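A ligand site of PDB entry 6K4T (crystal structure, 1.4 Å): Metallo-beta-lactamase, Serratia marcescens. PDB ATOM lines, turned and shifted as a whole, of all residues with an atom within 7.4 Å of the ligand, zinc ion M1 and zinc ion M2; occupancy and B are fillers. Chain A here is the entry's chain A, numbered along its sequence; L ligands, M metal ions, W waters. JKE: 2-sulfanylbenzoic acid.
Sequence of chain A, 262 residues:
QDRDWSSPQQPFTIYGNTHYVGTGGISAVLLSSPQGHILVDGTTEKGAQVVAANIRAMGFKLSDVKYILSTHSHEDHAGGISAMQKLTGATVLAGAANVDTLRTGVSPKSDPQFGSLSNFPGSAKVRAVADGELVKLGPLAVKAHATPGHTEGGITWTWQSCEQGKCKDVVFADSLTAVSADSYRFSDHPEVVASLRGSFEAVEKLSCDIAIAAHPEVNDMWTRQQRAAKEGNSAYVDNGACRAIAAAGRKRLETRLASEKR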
ATOM      1  N   TRP A   5     -26.689  25.512  34.078  1.00  0.00           N
ATOM      2  CA  TRP A   5     -25.945  24.307  34.438  1.00  0.00           C
ATOM      3  C   TRP A   5     -24.943  24.579  35.563  1.00  0.00           C
ATOM      4  O   TRP A   5     -24.489  23.678  36.234  1.00  0.00           O
ATOM      5  CB  TRP A   5     -25.156  23.764  33.255  1.00  0.00           C
ATOM      6  CG  TRP A   5     -25.970  23.194  32.146  1.00  0.00           C
ATOM      7  CD1 TRP A   5     -27.286  22.850  32.167  1.00  0.00           C
ATOM      8  CD2 TRP A   5     -25.480  22.894  30.835  1.00  0.00           C
ATOM      9  NE1 TRP A   5     -27.649  22.317  30.963  1.00  0.00           N
ATOM     10  CE2 TRP A   5     -26.567  22.347  30.119  1.00  0.00           C
ATOM     11  CE3 TRP A   5     -24.243  23.033  30.213  1.00  0.00           C
ATOM     12  CZ2 TRP A   5     -26.444  21.955  28.799  1.00  0.00           C
ATOM     13  CZ3 TRP A   5     -24.120  22.641  28.892  1.00  0.00           C
ATOM     14  CH2 TRP A   5     -25.209  22.102  28.207  1.00  0.00           C
ATOM     15  N   GLY A  25     -29.209  23.464  37.530  1.00  0.00           N
ATOM     16  CA  GLY A  25     -29.543  22.810  36.262  1.00  0.00           C
ATOM     17  C   GLY A  25     -28.964  21.408  36.076  1.00  0.00           C
ATOM     18  O   GLY A  25     -29.346  20.735  35.132  1.00  0.00           O
ATOM     19  N   ILE A  26     -27.991  21.007  36.904  1.00  0.00           N
ATOM     20  CA  ILE A  26     -27.358  19.704  36.766  1.00  0.00           C
ATOM     21  C   ILE A  26     -27.288  19.019  38.119  1.00  0.00           C
ATOM     22  O   ILE A  26     -26.799  19.584  39.105  1.00  0.00           O
ATOM     23  CB  ILE A  26     -25.943  19.770  36.140  1.00  0.00           C
ATOM     24  CG1 ILE A  26     -25.994  20.441  34.765  1.00  0.00           C
ATOM     25  CG2 ILE A  26     -25.313  18.397  36.077  1.00  0.00           C
ATOM     26  CD1 ILE A  26     -26.574  19.547  33.702  1.00  0.00           C
ATOM     27  N   HIS A  72     -22.033  10.150  32.734  1.00  0.00           N
ATOM     28  CA  HIS A  72     -21.403  10.144  31.454  1.00  0.00           C
ATOM     29  C   HIS A  72     -20.545  11.387  31.235  1.00  0.00           C
ATOM     30  O   HIS A  72     -20.667  12.390  31.933  1.00  0.00           O
ATOM     31  CB  HIS A  72     -22.431   9.975  30.330  1.00  0.00           C
ATOM     32  CG  HIS A  72     -23.280  11.178  30.035  1.00  0.00           C
ATOM     33  ND1 HIS A  72     -24.507  11.392  30.636  1.00  0.00           N
ATOM     34  CD2 HIS A  72     -23.096  12.209  29.174  1.00  0.00           C
ATOM     35  CE1 HIS A  72     -25.027  12.521  30.164  1.00  0.00           C
ATOM     36  NE2 HIS A  72     -24.182  13.039  29.249  1.00  0.00           N
ATOM     37  N   SER A  73     -19.706  11.267  30.201  1.00  0.00           N
ATOM     38  CA  SER A  73     -18.570  12.143  29.983  1.00  0.00           C
ATOM     39  C   SER A  73     -18.906  13.268  28.983  1.00  0.00           C
ATOM     40  O   SER A  73     -18.277  13.355  27.940  1.00  0.00           O
ATOM     41  CB  SER A  73     -17.407  11.315  29.520  1.00  0.00           C
ATOM     42  OG  SER A  73     -17.810  10.423  28.478  1.00  0.00           O
ATOM     43  N   HIS A  74     -19.898  14.099  29.326  1.00  0.00           N
ATOM     44  CA  HIS A  74     -20.091  15.398  28.653  1.00  0.00           C
ATOM     45  C   HIS A  74     -19.838  16.539  29.644  1.00  0.00           C
ATOM     46  O   HIS A  74     -19.932  16.361  30.866  1.00  0.00           O
ATOM     47  CB  HIS A  74     -21.499  15.515  28.046  1.00  0.00           C
ATOM     48  CG  HIS A  74     -21.716  14.563  26.929  1.00  0.00           C
ATOM     49  ND1 HIS A  74     -22.955  14.085  26.564  1.00  0.00           N
ATOM     50  CD2 HIS A  74     -20.826  13.974  26.106  1.00  0.00           C
ATOM     51  CE1 HIS A  74     -22.801  13.268  25.544  1.00  0.00           C
ATOM     52  NE2 HIS A  74     -21.515  13.162  25.255  1.00  0.00           N
ATOM     53  N   GLU A  75     -19.539  17.724  29.108  1.00  0.00           N
ATOM     54  CA  GLU A  75     -19.088  18.851  29.916  1.00  0.00           C
ATOM     55  C   GLU A  75     -20.096  19.195  31.030  1.00  0.00           C
ATOM     56  O   GLU A  75     -19.666  19.719  32.057  1.00  0.00           O
ATOM     57  CB  GLU A  75     -18.804  20.066  29.025  1.00  0.00           C
ATOM     58  CG  GLU A  75     -20.038  20.665  28.368  1.00  0.00           C
ATOM     59  CD  GLU A  75     -19.859  21.919  27.523  1.00  0.00           C
ATOM     60  OE1 GLU A  75     -19.081  22.779  27.926  1.00  0.00           O
ATOM     61  OE2 GLU A  75     -20.555  22.049  26.492  1.00  0.00           O
ATOM     62  N   ASP A  76     -21.395  18.986  30.814  1.00  0.00           N
ATOM     63  CA  ASP A  76     -22.385  19.471  31.759  1.00  0.00           C
ATOM     64  C   ASP A  76     -22.424  18.612  33.031  1.00  0.00           C
ATOM     65  O   ASP A  76     -22.762  19.125  34.077  1.00  0.00           O
ATOM     66  CB  ASP A  76     -23.748  19.651  31.084  1.00  0.00           C
ATOM     67  CG  ASP A  76     -24.303  18.419  30.385  1.00  0.00           C
ATOM     68  OD1 ASP A  76     -23.503  17.595  29.896  1.00  0.00           O
ATOM     69  OD2 ASP A  76     -25.560  18.278  30.377  1.00  0.00           O
ATOM     70  N   HIS A  77     -22.090  17.323  32.932  1.00  0.00           N
ATOM     71  CA  HIS A  77     -22.099  16.384  34.076  1.00  0.00           C
ATOM     72  C   HIS A  77     -20.683  16.198  34.647  1.00  0.00           C
ATOM     73  O   HIS A  77     -20.518  15.950  35.848  1.00  0.00           O
ATOM     74  CB  HIS A  77     -22.715  15.044  33.690  1.00  0.00           C
ATOM     75  CG  HIS A  77     -24.027  15.227  32.987  1.00  0.00           C
ATOM     76  ND1 HIS A  77     -25.212  15.482  33.691  1.00  0.00           N
ATOM     77  CD2 HIS A  77     -24.328  15.272  31.672  1.00  0.00           C
ATOM     78  CE1 HIS A  77     -26.178  15.660  32.800  1.00  0.00           C
ATOM     79  NE2 HIS A  77     -25.670  15.582  31.549  1.00  0.00           N
ATOM     80  N   ASP A 111     -19.397   8.988  19.684  1.00  0.00           N
ATOM     81  CA  ASP A 111     -20.456   9.739  20.348  1.00  0.00           C
ATOM     82  C   ASP A 111     -21.360  10.379  19.293  1.00  0.00           C
ATOM     83  O   ASP A 111     -20.868  11.071  18.419  1.00  0.00           O
ATOM     84  CB  ASP A 111     -19.845  10.760  21.298  1.00  0.00           C
ATOM     85  CG  ASP A 111     -20.831  11.443  22.228  1.00  0.00           C
ATOM     86  OD1 ASP A 111     -21.875  11.929  21.741  1.00  0.00           O
ATOM     87  OD2 ASP A 111     -20.509  11.536  23.411  1.00  0.00           O
ATOM     88  N   GLN A 113     -23.004  12.978  19.299  1.00  0.00           N
ATOM     89  CA  GLN A 113     -22.826  14.433  19.292  1.00  0.00           C
ATOM     90  C   GLN A 113     -21.442  14.842  18.806  1.00  0.00           C
ATOM     91  O   GLN A 113     -21.170  16.037  18.705  1.00  0.00           O
ATOM     92  CB  GLN A 113     -23.108  15.017  20.676  1.00  0.00           C
ATOM     93  CG  GLN A 113     -24.587  14.929  21.055  1.00  0.00           C
ATOM     94  CD  GLN A 113     -24.821  15.500  22.429  1.00  0.00           C
ATOM     95  OE1 GLN A 113     -24.836  14.789  23.437  1.00  0.00           O
ATOM     96  NE2 GLN A 113     -24.907  16.813  22.497  1.00  0.00           N
ATOM     97  N   LEU A 117     -19.653  18.816  20.355  1.00  0.00           N
ATOM     98  CA  LEU A 117     -19.410  18.831  21.795  1.00  0.00           C
ATOM     99  C   LEU A 117     -18.289  19.812  22.139  1.00  0.00           C
ATOM    100  O   LEU A 117     -17.371  20.012  21.356  1.00  0.00           O
ATOM    101  CB  LEU A 117     -19.050  17.418  22.282  1.00  0.00           C
ATOM    102  CG  LEU A 117     -20.217  16.422  22.238  1.00  0.00           C
ATOM    103  CD1 LEU A 117     -19.716  14.978  22.284  1.00  0.00           C
ATOM    104  CD2 LEU A 117     -21.197  16.688  23.363  1.00  0.00           C
ATOM    105  N   HIS A 150     -26.454   7.102  24.964  1.00  0.00           N
ATOM    106  CA  HIS A 150     -26.093   8.526  24.949  1.00  0.00           C
ATOM    107  C   HIS A 150     -24.577   8.672  24.871  1.00  0.00           C
ATOM    108  O   HIS A 150     -24.077   9.538  24.157  1.00  0.00           O
ATOM    109  CB  HIS A 150     -26.760   9.240  26.139  1.00  0.00           C
ATOM    110  CG  HIS A 150     -26.520  10.705  26.199  1.00  0.00           C
ATOM    111  ND1 HIS A 150     -27.277  11.610  25.478  1.00  0.00           N
ATOM    112  CD2 HIS A 150     -25.642  11.440  26.914  1.00  0.00           C
ATOM    113  CE1 HIS A 150     -26.880  12.845  25.767  1.00  0.00           C
ATOM    114  NE2 HIS A 150     -25.880  12.763  26.653  1.00  0.00           N
ATOM    115  N   THR A 151     -23.876   7.784  25.597  1.00  0.00           N
ATOM    116  CA  THR A 151     -22.416   7.570  25.469  1.00  0.00           C
ATOM    117  C   THR A 151     -22.173   6.073  25.634  1.00  0.00           C
ATOM    118  O   THR A 151     -23.019   5.381  26.219  1.00  0.00           O
ATOM    119  CB  THR A 151     -21.602   8.349  26.510  1.00  0.00           C
ATOM    120  OG1 THR A 151     -21.882   7.801  27.807  1.00  0.00           O
ATOM    121  CG2 THR A 151     -21.835   9.842  26.478  1.00  0.00           C
ATOM    122  N   ASP A 174     -28.617   8.041  34.650  1.00  0.00           N
ATOM    123  CA  ASP A 174     -27.910   8.613  33.519  1.00  0.00           C
ATOM    124  C   ASP A 174     -28.923   9.025  32.439  1.00  0.00           C
ATOM    125  O   ASP A 174     -30.085   8.576  32.416  1.00  0.00           O
ATOM    126  CB  ASP A 174     -26.897   7.638  32.958  1.00  0.00           C
ATOM    127  CG  ASP A 174     -25.937   8.262  31.960  1.00  0.00           C
ATOM    128  OD1 ASP A 174     -25.768   9.498  32.010  1.00  0.00           O
ATOM    129  OD2 ASP A 174     -25.281   7.479  31.235  1.00  0.00           O
ATOM    130  N   SER A 175     -28.474   9.947  31.589  1.00  0.00           N
ATOM    131  CA  SER A 175     -29.239  10.358  30.420  1.00  0.00           C
ATOM    132  C   SER A 175     -29.406   9.201  29.435  1.00  0.00           C
ATOM    133  O   SER A 175     -28.461   8.483  29.140  1.00  0.00           O
ATOM    134  CB  SER A 175     -28.559  11.532  29.781  1.00  0.00           C
ATOM    135  OG  SER A 175     -28.431  12.584  30.728  1.00  0.00           O
ATOM    136  N   LEU A 176     -30.618   9.050  28.892  1.00  0.00           N
ATOM    137  CA  LEU A 176     -30.956   8.025  27.934  1.00  0.00           C
ATOM    138  C   LEU A 176     -31.373   8.650  26.599  1.00  0.00           C
ATOM    139  O   LEU A 176     -32.200   8.079  25.867  1.00  0.00           O
ATOM    140  CB  LEU A 176     -32.112   7.204  28.513  1.00  0.00           C
ATOM    141  CG  LEU A 176     -31.882   6.547  29.870  1.00  0.00           C
ATOM    142  CD1 LEU A 176     -33.082   5.723  30.307  1.00  0.00           C
ATOM    143  CD2 LEU A 176     -30.625   5.694  29.836  1.00  0.00           C
ATOM    144  N   THR A 177     -30.879   9.851  26.304  1.00  0.00           N
ATOM    145  CA  THR A 177     -31.395  10.667  25.230  1.00  0.00           C
ATOM    146  C   THR A 177     -30.607  10.490  23.923  1.00  0.00           C
ATOM    147  O   THR A 177     -29.395  10.574  23.847  1.00  0.00           O
ATOM    148  CB  THR A 177     -31.332  12.135  25.647  1.00  0.00           C
ATOM    149  OG1 THR A 177     -29.971  12.429  26.000  1.00  0.00           O
ATOM    150  CG2 THR A 177     -32.255  12.451  26.806  1.00  0.00           C
ATOM    151  N   ALA A 178     -31.375  10.290  22.845  1.00  0.00           N
ATOM    152  CA  ALA A 178     -30.895  10.318  21.468  1.00  0.00           C
ATOM    153  C   ALA A 178     -30.806  11.766  21.002  1.00  0.00           C
ATOM    154  O   ALA A 178     -31.847  12.437  20.759  1.00  0.00           O
ATOM    155  CB  ALA A 178     -31.812   9.493  20.592  1.00  0.00           C
ATOM    156  N   VAL A 179     -29.574  12.257  20.919  1.00  0.00           N
ATOM    157  CA  VAL A 179     -29.269  13.617  20.459  1.00  0.00           C
ATOM    158  C   VAL A 179     -27.970  13.511  19.655  1.00  0.00           C
ATOM    159  O   VAL A 179     -27.135  12.715  19.965  1.00  0.00           O
ATOM    160  CB  VAL A 179     -29.143  14.598  21.656  1.00  0.00           C
ATOM    161  CG1 VAL A 179     -28.203  14.092  22.725  1.00  0.00           C
ATOM    162  CG2 VAL A 179     -28.744  16.006  21.246  1.00  0.00           C
ATOM    163  N   SER A 180     -27.795  14.365  18.658  1.00  0.00           N
ATOM    164  CA  SER A 180     -26.630  14.200  17.781  1.00  0.00           C
ATOM    165  C   SER A 180     -26.237  15.508  17.100  1.00  0.00           C
ATOM    166  O   SER A 180     -27.023  16.472  17.049  1.00  0.00           O
ATOM    167  CB  SER A 180     -26.869  13.139  16.726  1.00  0.00           C
ATOM    168  OG  SER A 180     -27.721  13.646  15.691  1.00  0.00           O
ATOM    169  N   ALA A 214     -29.909  12.906  35.892  1.00  0.00           N
ATOM    170  CA  ALA A 214     -28.710  13.725  35.700  1.00  0.00           C
ATOM    171  C   ALA A 214     -29.088  15.179  35.340  1.00  0.00           C
ATOM    172  O   ALA A 214     -28.502  16.128  35.872  1.00  0.00           O
ATOM    173  CB  ALA A 214     -27.840  13.105  34.629  1.00  0.00           C
ATOM    174  N   HIS A 215     -30.067  15.339  34.440  1.00  0.00           N
ATOM    175  CA  HIS A 215     -30.795  16.586  34.277  1.00  0.00           C
ATOM    176  C   HIS A 215     -31.997  16.556  35.213  1.00  0.00           C
ATOM    177  O   HIS A 215     -32.926  15.791  34.954  1.00  0.00           O
ATOM    178  CB  HIS A 215     -31.224  16.787  32.810  1.00  0.00           C
ATOM    179  CG  HIS A 215     -30.056  17.118  31.927  1.00  0.00           C
ATOM    180  ND1 HIS A 215     -29.588  18.408  31.803  1.00  0.00           N
ATOM    181  CD2 HIS A 215     -29.220  16.341  31.200  1.00  0.00           C
ATOM    182  CE1 HIS A 215     -28.525  18.419  31.030  1.00  0.00           C
ATOM    183  NE2 HIS A 215     -28.277  17.158  30.620  1.00  0.00           N
ATOM    184  N   VAL A 218     -35.788  16.134  34.449  1.00  0.00           N
ATOM    185  CA  VAL A 218     -36.237  14.931  33.790  1.00  0.00           C
ATOM    186  C   VAL A 218     -37.221  14.165  34.678  1.00  0.00           C
ATOM    187  O   VAL A 218     -38.174  13.575  34.172  1.00  0.00           O
ATOM    188  CB  VAL A 218     -35.047  14.066  33.319  1.00  0.00           C
ATOM    189  CG1 VAL A 218     -35.442  12.620  33.053  1.00  0.00           C
ATOM    190  CG2 VAL A 218     -34.443  14.667  32.066  1.00  0.00           C
ATOM    191  N   ARG A 252     -38.229   9.481  22.612  1.00  0.00           N
ATOM    192  CA  ARG A 252     -37.298  10.353  21.912  1.00  0.00           C
ATOM    193  C   ARG A 252     -36.600   9.604  20.773  1.00  0.00           C
ATOM    194  O   ARG A 252     -36.441  10.120  19.662  1.00  0.00           O
ATOM    195  CB  ARG A 252     -36.281  10.911  22.897  1.00  0.00           C
ATOM    196  CG  ARG A 252     -35.321  11.945  22.311  1.00  0.00           C
ATOM    197  CD  ARG A 252     -34.573  12.658  23.413  1.00  0.00           C
ATOM    198  NE  ARG A 252     -33.626  13.613  22.846  1.00  0.00           N
ATOM    199  CZ  ARG A 252     -33.246  14.759  23.421  1.00  0.00           C
ATOM    200  NH1 ARG A 252     -33.619  15.022  24.666  1.00  0.00           N
ATOM    201  NH2 ARG A 252     -32.425  15.578  22.806  1.00  0.00           N
HETATM  202  SD  JKE L   1     -25.617  16.239  27.769  1.00  0.00           S
HETATM  203  CG  JKE L   1     -28.511  14.741  28.200  1.00  0.00           C
HETATM  204  CZ  JKE L   1     -28.277  15.656  27.061  1.00  0.00           C
HETATM  205  CD1 JKE L   1     -26.937  17.173  25.638  1.00  0.00           C
HETATM  206  OD1 JKE L   1     -29.554  14.090  28.183  1.00  0.00           O
HETATM  207  CD2 JKE L   1     -29.233  16.713  25.099  1.00  0.00           C
HETATM  208  OD2 JKE L   1     -27.671  14.624  29.189  1.00  0.00           O
HETATM  209  CE1 JKE L   1     -27.019  16.343  26.764  1.00  0.00           C
HETATM  210  CE2 JKE L   1     -29.353  15.884  26.210  1.00  0.00           C
HETATM  211  CG1 JKE L   1     -28.039  17.349  24.800  1.00  0.00           C
HETATM  212 ZN    ZN M   1     -24.761  14.169  27.644  1.00  0.00          ZN
HETATM  213 ZN    ZN M   2     -26.447  16.476  29.947  1.00  0.00          ZN
HETATM  214  O   HOH W   1     -30.509  18.411  28.206  1.00  0.00           O
HETATM  215  O   HOH W   2     -31.717  13.524  29.927  1.00  0.00           O
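An oxygen (OD1) of the ligand is in hydrogen-bond range of the side-chain hydroxyl (OG1) of Thr 177, at 2.8 Å. The side-chain hydroxyl (OG) of Ser 175 sits at hydrogen-bond distance from an oxygen (OD1) of the ligand (3.2 Å).
Of the 25 residues printed, 3 come within 4 Å of zinc ion M1.
Zinc ion M1 is bound by NE2 of His 72 (2.0 Å). A ring nitrogen (NE2) of His 150 binds zinc ion M1. Zinc ion M1 is bound by a ring nitrogen (ND1) of His 74 (2.1 Å). Zinc ion M1 is bound by SD of the ligand, at 2.2 Å. Zinc ion M1 has four donor atoms within binding distance.
Zinc ion M2 is bound by a ring nitrogen (NE2) of His 77 (2.0 Å), the side-chain carboxylate of Asp 76 (2.1 Å), a ring nitrogen (NE2) of His 215 (2.1 Å), a sulfur (SD) of the ligand (2.3 Å) and an oxygen (OD2) of the ligand (2.3 Å). Zinc ion M2 has five donor atoms within binding distance.
NE2 of His 74 is in hydrogen-bond range of OD2 of Asp 111. N of Gln 113 is in hydrogen-bond range of OD1 of Asp 111 (2.9 Å). OG1 of Thr 177 is in hydrogen-bond range of ND1 of His 150 (2.9 Å). ND1 of His 72 lies within hydrogen-bond range of OD1 of Asp 174.
Gln 113 touches the ligand (NE2 to CD1, 3.8 Å). Val 179 touches the ligand (CG1 to CD2, 3.7 Å). Hydrophobic or aromatic side chains that line the ligand: His 72, His 150, Val 179 and His 215. Of the 25 residues printed, 10 come within 4 Å of the ligand. Along chain A the residues within 4 Å of the ligand span positions 72 to 215. The nearest printed residue that does not touch the ligand is Arg 252 (4.1 Å).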
